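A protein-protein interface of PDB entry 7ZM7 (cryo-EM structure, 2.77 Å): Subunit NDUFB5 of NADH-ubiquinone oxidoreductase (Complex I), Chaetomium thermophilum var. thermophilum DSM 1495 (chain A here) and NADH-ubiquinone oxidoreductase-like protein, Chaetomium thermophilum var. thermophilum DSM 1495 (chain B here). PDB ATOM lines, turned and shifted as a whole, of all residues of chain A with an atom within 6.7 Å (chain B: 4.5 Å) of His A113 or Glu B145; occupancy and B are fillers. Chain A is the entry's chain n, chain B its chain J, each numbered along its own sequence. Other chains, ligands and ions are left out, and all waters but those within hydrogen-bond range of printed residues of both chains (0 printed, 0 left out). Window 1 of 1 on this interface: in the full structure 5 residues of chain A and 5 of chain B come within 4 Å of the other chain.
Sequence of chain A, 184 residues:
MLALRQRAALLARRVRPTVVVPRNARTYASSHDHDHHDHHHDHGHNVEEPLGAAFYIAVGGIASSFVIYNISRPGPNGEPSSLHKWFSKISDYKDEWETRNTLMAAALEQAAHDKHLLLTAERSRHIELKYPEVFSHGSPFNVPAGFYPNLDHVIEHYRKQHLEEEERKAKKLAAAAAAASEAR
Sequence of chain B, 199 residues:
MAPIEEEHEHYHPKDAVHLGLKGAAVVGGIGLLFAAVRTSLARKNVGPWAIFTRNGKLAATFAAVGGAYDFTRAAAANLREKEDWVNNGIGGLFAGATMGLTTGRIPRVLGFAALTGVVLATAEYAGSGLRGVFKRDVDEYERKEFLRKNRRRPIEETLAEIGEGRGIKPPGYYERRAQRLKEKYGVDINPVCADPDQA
OE2 of Glu A109 lies within salt-bridge range of NH2 of Arg B148, at 3.4 Å.
OE1 of Glu B145 lies within hydrogen-bond range of ND1 of His A113, at 3.5 Å.
The side-chain carboxylate (OE2) of Glu B145 is in hydrogen-bond range of a ring nitrogen (ND1) of His A116 (2.9 Å).
Of chain B, only Tyr B141, Glu B145 and Arg B148 come within 4 Å of His A113.
Glu B145 touches just these residues of chain A: His A113 and His A116.
Of the printed residues of chain A, Lys B144 touches His A116.
Printed residues of chain B within 4 Å of His A116: Lys B144 and Glu B145.
Printed residues of chain A within 4 Å of Arg B148: Glu A109 (3.4 Å) and His A113 (3.8 Å).
Leu A108 touches none of the printed residues of chain B.
The nearest printed residue of chain B that does not touch His A113 is Lys B149 (6.0 Å).
The nearest residue of chain A that does not touch Glu B145 is Ala A112 (4.6 Å).
The side-chain carboxylate of Glu B145 is in salt-bridge range of the side-chain amino group of Lys B149.
The side-chain carboxylate (OE2) of Glu B145 lies within salt-bridge range of the guanidinium group (NE) of Arg B148 (2.8 Å).
Of the 9 printed residues of chain B, 4 touch a printed residue of chain A.
Hydrophobic or aromatic side chains of chain B that line the printed part of chain A: Tyr B141.
Printed residues of chain A that touch a printed residue of chain B: Glu A109, His A113, His A116 and Leu A117.
Among the printed residues, 7 pairs touch across the chains.
CE1 of His A113 touches OH of Tyr B141 (3.1 Å).
Arg B148 touches His A113 (NH1 to CB, 3.8 Å).
O of Lys B144 touches CE1 of His A116, at 3.9 Å.
Leu A117 touches Tyr B141 (CD1 to CE1, 3.8 Å).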
ATOM      1  N   LEU A 108     -10.531 -13.022 -17.399  1.00  0.00           N
ATOM      2  CA  LEU A 108     -10.763 -14.411 -17.057  1.00  0.00           C
ATOM      3  C   LEU A 108      -9.569 -15.017 -16.333  1.00  0.00           C
ATOM      4  O   LEU A 108      -9.749 -15.952 -15.549  1.00  0.00           O
ATOM      5  CB  LEU A 108     -11.148 -15.186 -18.313  1.00  0.00           C
ATOM      6  CG  LEU A 108     -12.583 -14.821 -18.723  1.00  0.00           C
ATOM      7  CD1 LEU A 108     -12.831 -15.028 -20.192  1.00  0.00           C
ATOM      8  CD2 LEU A 108     -13.611 -15.577 -17.911  1.00  0.00           C
ATOM      9  N   GLU A 109      -8.359 -14.493 -16.550  1.00  0.00           N
ATOM     10  CA  GLU A 109      -7.260 -14.765 -15.625  1.00  0.00           C
ATOM     11  C   GLU A 109      -7.533 -14.202 -14.238  1.00  0.00           C
ATOM     12  O   GLU A 109      -7.126 -14.794 -13.234  1.00  0.00           O
ATOM     13  CB  GLU A 109      -5.940 -14.197 -16.142  1.00  0.00           C
ATOM     14  CG  GLU A 109      -5.411 -14.748 -17.439  1.00  0.00           C
ATOM     15  CD  GLU A 109      -4.714 -16.079 -17.259  1.00  0.00           C
ATOM     16  OE1 GLU A 109      -4.503 -16.787 -18.266  1.00  0.00           O
ATOM     17  OE2 GLU A 109      -4.374 -16.412 -16.109  1.00  0.00           O
ATOM     18  N   GLN A 110      -8.181 -13.041 -14.162  1.00  0.00           N
ATOM     19  CA  GLN A 110      -8.399 -12.405 -12.871  1.00  0.00           C
ATOM     20  C   GLN A 110      -9.397 -13.188 -12.032  1.00  0.00           C
ATOM     21  O   GLN A 110      -9.247 -13.292 -10.811  1.00  0.00           O
ATOM     22  CB  GLN A 110      -8.880 -10.975 -13.071  1.00  0.00           C
ATOM     23  CG  GLN A 110      -9.063 -10.193 -11.791  1.00  0.00           C
ATOM     24  CD  GLN A 110      -7.771 -10.023 -11.020  1.00  0.00           C
ATOM     25  OE1 GLN A 110      -7.545 -10.680 -10.005  1.00  0.00           O
ATOM     26  NE2 GLN A 110      -6.914  -9.132 -11.499  1.00  0.00           N
ATOM     27  N   ALA A 111     -10.429 -13.742 -12.669  1.00  0.00           N
ATOM     28  CA  ALA A 111     -11.419 -14.507 -11.934  1.00  0.00           C
ATOM     29  C   ALA A 111     -10.966 -15.936 -11.697  1.00  0.00           C
ATOM     30  O   ALA A 111     -11.526 -16.626 -10.844  1.00  0.00           O
ATOM     31  CB  ALA A 111     -12.750 -14.477 -12.670  1.00  0.00           C
ATOM     32  N   ALA A 112      -9.990 -16.416 -12.460  1.00  0.00           N
ATOM     33  CA  ALA A 112      -9.331 -17.662 -12.090  1.00  0.00           C
ATOM     34  C   ALA A 112      -8.620 -17.511 -10.755  1.00  0.00           C
ATOM     35  O   ALA A 112      -8.664 -18.409  -9.909  1.00  0.00           O
ATOM     36  CB  ALA A 112      -8.349 -18.080 -13.176  1.00  0.00           C
ATOM     37  N   HIS A 113      -7.994 -16.354 -10.535  1.00  0.00           N
ATOM     38  CA  HIS A 113      -7.292 -16.098  -9.253  1.00  0.00           C
ATOM     39  C   HIS A 113      -8.319 -15.866  -8.148  1.00  0.00           C
ATOM     40  O   HIS A 113      -8.100 -16.378  -7.029  1.00  0.00           O
ATOM     41  CB  HIS A 113      -6.351 -14.893  -9.387  1.00  0.00           C
ATOM     42  CG  HIS A 113      -6.165 -14.139  -8.116  1.00  0.00           C
ATOM     43  ND1 HIS A 113      -5.372 -14.606  -7.089  1.00  0.00           N
ATOM     44  CD2 HIS A 113      -6.672 -12.959  -7.696  1.00  0.00           C
ATOM     45  CE1 HIS A 113      -5.398 -13.747  -6.091  1.00  0.00           C
ATOM     46  NE2 HIS A 113      -6.189 -12.727  -6.438  1.00  0.00           N
ATOM     47  N   ASP A 114      -9.401 -15.140  -8.443  1.00  0.00           N
ATOM     48  CA  ASP A 114     -10.358 -14.785  -7.406  1.00  0.00           C
ATOM     49  C   ASP A 114     -11.157 -15.972  -6.913  1.00  0.00           C
ATOM     50  O   ASP A 114     -11.574 -15.978  -5.755  1.00  0.00           O
ATOM     51  CB  ASP A 114     -11.320 -13.722  -7.912  1.00  0.00           C
ATOM     52  CG  ASP A 114     -10.854 -12.334  -7.604  1.00  0.00           C
ATOM     53  OD1 ASP A 114      -9.790 -12.191  -6.976  1.00  0.00           O
ATOM     54  OD2 ASP A 114     -11.560 -11.379  -7.980  1.00  0.00           O
ATOM     55  N   LYS A 115     -11.388 -16.960  -7.769  1.00  0.00           N
ATOM     56  CA  LYS A 115     -12.139 -18.135  -7.362  1.00  0.00           C
ATOM     57  C   LYS A 115     -11.288 -19.056  -6.502  1.00  0.00           C
ATOM     58  O   LYS A 115     -11.797 -19.676  -5.565  1.00  0.00           O
ATOM     59  CB  LYS A 115     -12.671 -18.849  -8.601  1.00  0.00           C
ATOM     60  CG  LYS A 115     -12.890 -20.314  -8.446  1.00  0.00           C
ATOM     61  CD  LYS A 115     -13.063 -20.950  -9.790  1.00  0.00           C
ATOM     62  CE  LYS A 115     -12.980 -22.454  -9.708  1.00  0.00           C
ATOM     63  NZ  LYS A 115     -13.247 -23.070 -11.035  1.00  0.00           N
ATOM     64  N   HIS A 116      -9.989 -19.151  -6.791  1.00  0.00           N
ATOM     65  CA  HIS A 116      -9.080 -19.819  -5.865  1.00  0.00           C
ATOM     66  C   HIS A 116      -9.073 -19.143  -4.503  1.00  0.00           C
ATOM     67  O   HIS A 116      -9.057 -19.816  -3.473  1.00  0.00           O
ATOM     68  CB  HIS A 116      -7.664 -19.854  -6.433  1.00  0.00           C
ATOM     69  CG  HIS A 116      -7.441 -20.904  -7.471  1.00  0.00           C
ATOM     70  ND1 HIS A 116      -6.295 -20.963  -8.227  1.00  0.00           N
ATOM     71  CD2 HIS A 116      -8.182 -21.972  -7.832  1.00  0.00           C
ATOM     72  CE1 HIS A 116      -6.352 -22.008  -9.028  1.00  0.00           C
ATOM     73  NE2 HIS A 116      -7.487 -22.638  -8.807  1.00  0.00           N
ATOM     74  N   LEU A 117      -9.004 -17.822  -4.455  1.00  0.00           N
ATOM     75  CA  LEU A 117      -8.931 -17.081  -3.168  1.00  0.00           C
ATOM     76  C   LEU A 117     -10.191 -17.339  -2.343  1.00  0.00           C
ATOM     77  O   LEU A 117     -10.068 -17.642  -1.159  1.00  0.00           O
ATOM     78  CB  LEU A 117      -8.790 -15.597  -3.499  1.00  0.00           C
ATOM     79  CG  LEU A 117      -8.693 -14.645  -2.312  1.00  0.00           C
ATOM     80  CD1 LEU A 117      -7.333 -14.758  -1.643  1.00  0.00           C
ATOM     81  CD2 LEU A 117      -8.943 -13.221  -2.770  1.00  0.00           C
ATOM     82  N   LEU A 118     -11.354 -17.266  -2.916  1.00  0.00           N
ATOM     83  CA  LEU A 118     -12.614 -17.425  -2.156  1.00  0.00           C
ATOM     84  C   LEU A 118     -12.853 -18.892  -1.794  1.00  0.00           C
ATOM     85  O   LEU A 118     -13.382 -19.137  -0.708  1.00  0.00           O
ATOM     86  CB  LEU A 118     -13.768 -16.847  -2.972  1.00  0.00           C
ATOM     87  CG  LEU A 118     -13.841 -15.327  -3.067  1.00  0.00           C
ATOM     88  CD1 LEU A 118     -14.599 -14.910  -4.317  1.00  0.00           C
ATOM     89  CD2 LEU A 118     -14.497 -14.738  -1.832  1.00  0.00           C
ATOM     90  N   TYR B 141      -4.325 -22.339  -0.996  1.00  0.00           N
ATOM     91  CA  TYR B 141      -4.164 -21.186  -1.919  1.00  0.00           C
ATOM     92  C   TYR B 141      -2.787 -21.239  -2.560  1.00  0.00           C
ATOM     93  O   TYR B 141      -2.690 -21.080  -3.778  1.00  0.00           O
ATOM     94  CB  TYR B 141      -4.396 -19.854  -1.215  1.00  0.00           C
ATOM     95  CG  TYR B 141      -4.129 -18.618  -2.034  1.00  0.00           C
ATOM     96  CD1 TYR B 141      -5.120 -18.040  -2.810  1.00  0.00           C
ATOM     97  CD2 TYR B 141      -2.884 -18.015  -2.020  1.00  0.00           C
ATOM     98  CE1 TYR B 141      -4.876 -16.902  -3.559  1.00  0.00           C
ATOM     99  CE2 TYR B 141      -2.625 -16.875  -2.755  1.00  0.00           C
ATOM    100  CZ  TYR B 141      -3.623 -16.315  -3.526  1.00  0.00           C
ATOM    101  OH  TYR B 141      -3.348 -15.194  -4.250  1.00  0.00           O
ATOM    102  N   GLU B 142      -1.758 -21.525  -1.774  1.00  0.00           N
ATOM    103  CA  GLU B 142      -0.409 -21.683  -2.375  1.00  0.00           C
ATOM    104  C   GLU B 142      -0.372 -22.894  -3.310  1.00  0.00           C
ATOM    105  O   GLU B 142       0.205 -22.759  -4.395  1.00  0.00           O
ATOM    106  CB  GLU B 142       0.666 -21.726  -1.293  1.00  0.00           C
ATOM    107  CG  GLU B 142       1.224 -20.355  -0.966  1.00  0.00           C
ATOM    108  CD  GLU B 142       2.089 -20.301   0.279  1.00  0.00           C
ATOM    109  OE1 GLU B 142       2.594 -19.208   0.598  1.00  0.00           O
ATOM    110  OE2 GLU B 142       2.253 -21.353   0.928  1.00  0.00           O
ATOM    111  N   ARG B 143      -0.956 -24.024  -2.908  1.00  0.00           N
ATOM    112  CA  ARG B 143      -0.853 -25.261  -3.731  1.00  0.00           C
ATOM    113  C   ARG B 143      -1.575 -25.076  -5.068  1.00  0.00           C
ATOM    114  O   ARG B 143      -0.987 -25.416  -6.106  1.00  0.00           O
ATOM    115  CB  ARG B 143      -1.397 -26.455  -2.946  1.00  0.00           C
ATOM    116  CG  ARG B 143      -1.545 -27.728  -3.764  1.00  0.00           C
ATOM    117  CD  ARG B 143      -2.051 -28.878  -2.918  1.00  0.00           C
ATOM    118  NE  ARG B 143      -2.428 -30.029  -3.724  1.00  0.00           N
ATOM    119  CZ  ARG B 143      -1.612 -31.028  -4.040  1.00  0.00           C
ATOM    120  NH1 ARG B 143      -0.360 -31.023  -3.618  1.00  0.00           N
ATOM    121  NH2 ARG B 143      -2.054 -32.030  -4.778  1.00  0.00           N
ATOM    122  N   LYS B 144      -2.788 -24.520  -5.031  1.00  0.00           N
ATOM    123  CA  LYS B 144      -3.588 -24.309  -6.258  1.00  0.00           C
ATOM    124  C   LYS B 144      -2.914 -23.255  -7.130  1.00  0.00           C
ATOM    125  O   LYS B 144      -2.808 -23.485  -8.338  1.00  0.00           O
ATOM    126  CB  LYS B 144      -5.025 -23.960  -5.869  1.00  0.00           C
ATOM    127  CG  LYS B 144      -5.953 -25.141  -5.628  1.00  0.00           C
ATOM    128  CD  LYS B 144      -6.315 -25.874  -6.901  1.00  0.00           C
ATOM    129  CE  LYS B 144      -7.502 -26.799  -6.734  1.00  0.00           C
ATOM    130  NZ  LYS B 144      -7.266 -27.819  -5.685  1.00  0.00           N
ATOM    131  N   GLU B 145      -2.452 -22.165  -6.525  1.00  0.00           N
ATOM    132  CA  GLU B 145      -1.843 -21.052  -7.302  1.00  0.00           C
ATOM    133  C   GLU B 145      -0.528 -21.488  -7.950  1.00  0.00           C
ATOM    134  O   GLU B 145      -0.242 -21.021  -9.060  1.00  0.00           O
ATOM    135  CB  GLU B 145      -1.755 -19.770  -6.475  1.00  0.00           C
ATOM    136  CG  GLU B 145      -3.078 -19.046  -6.325  1.00  0.00           C
ATOM    137  CD  GLU B 145      -3.529 -18.282  -7.555  1.00  0.00           C
ATOM    138  OE1 GLU B 145      -3.079 -17.139  -7.731  1.00  0.00           O
ATOM    139  OE2 GLU B 145      -4.325 -18.830  -8.334  1.00  0.00           O
ATOM    140  N   PHE B 146       0.258 -22.318  -7.269  1.00  0.00           N
ATOM    141  CA  PHE B 146       1.508 -22.832  -7.877  1.00  0.00           C
ATOM    142  C   PHE B 146       1.181 -23.664  -9.108  1.00  0.00           C
ATOM    143  O   PHE B 146       1.860 -23.508 -10.121  1.00  0.00           O
ATOM    144  CB  PHE B 146       2.310 -23.700  -6.909  1.00  0.00           C
ATOM    145  CG  PHE B 146       3.500 -24.364  -7.550  1.00  0.00           C
ATOM    146  CD1 PHE B 146       4.607 -23.622  -7.926  1.00  0.00           C
ATOM    147  CD2 PHE B 146       3.504 -25.726  -7.807  1.00  0.00           C
ATOM    148  CE1 PHE B 146       5.695 -24.225  -8.535  1.00  0.00           C
ATOM    149  CE2 PHE B 146       4.590 -26.327  -8.419  1.00  0.00           C
ATOM    150  CZ  PHE B 146       5.685 -25.578  -8.779  1.00  0.00           C
ATOM    151  N   LEU B 147       0.156 -24.504  -9.028  1.00  0.00           N
ATOM    152  CA  LEU B 147      -0.116 -25.412 -10.163  1.00  0.00           C
ATOM    153  C   LEU B 147      -0.811 -24.654 -11.300  1.00  0.00           C
ATOM    154  O   LEU B 147      -0.874 -25.205 -12.392  1.00  0.00           O
ATOM    155  CB  LEU B 147      -0.918 -26.602  -9.634  1.00  0.00           C
ATOM    156  CG  LEU B 147      -0.144 -27.586  -8.764  1.00  0.00           C
ATOM    157  CD1 LEU B 147      -1.058 -28.694  -8.276  1.00  0.00           C
ATOM    158  CD2 LEU B 147       1.029 -28.168  -9.532  1.00  0.00           C
ATOM    159  N   ARG B 148      -1.287 -23.434 -11.060  1.00  0.00           N
ATOM    160  CA  ARG B 148      -1.900 -22.600 -12.129  1.00  0.00           C
ATOM    161  C   ARG B 148      -0.816 -21.768 -12.832  1.00  0.00           C
ATOM    162  O   ARG B 148      -0.905 -21.594 -14.057  1.00  0.00           O
ATOM    163  CB  ARG B 148      -2.956 -21.668 -11.517  1.00  0.00           C
ATOM    164  CG  ARG B 148      -3.556 -20.680 -12.509  1.00  0.00           C
ATOM    165  CD  ARG B 148      -4.586 -19.720 -11.947  1.00  0.00           C
ATOM    166  NE  ARG B 148      -4.054 -18.642 -11.128  1.00  0.00           N
ATOM    167  CZ  ARG B 148      -3.711 -17.446 -11.586  1.00  0.00           C
ATOM    168  NH1 ARG B 148      -3.243 -16.531 -10.758  1.00  0.00           N
ATOM    169  NH2 ARG B 148      -3.835 -17.165 -12.869  1.00  0.00           N
ATOM    170  N   LYS B 149       0.167 -21.272 -12.087  1.00  0.00           N
ATOM    171  CA  LYS B 149       1.227 -20.458 -12.652  1.00  0.00           C
ATOM    172  C   LYS B 149       2.514 -21.225 -12.898  1.00  0.00           C
ATOM    173  O   LYS B 149       3.545 -20.607 -13.162  1.00  0.00           O
ATOM    174  CB  LYS B 149       1.480 -19.247 -11.765  1.00  0.00           C
ATOM    175  CG  LYS B 149       0.311 -18.308 -11.717  1.00  0.00           C
ATOM    176  CD  LYS B 149       0.647 -17.058 -10.930  1.00  0.00           C
ATOM    177  CE  LYS B 149       0.770 -17.324  -9.446  1.00  0.00           C
ATOM    178  NZ  LYS B 149      -0.523 -17.679  -8.853  1.00  0.00           N
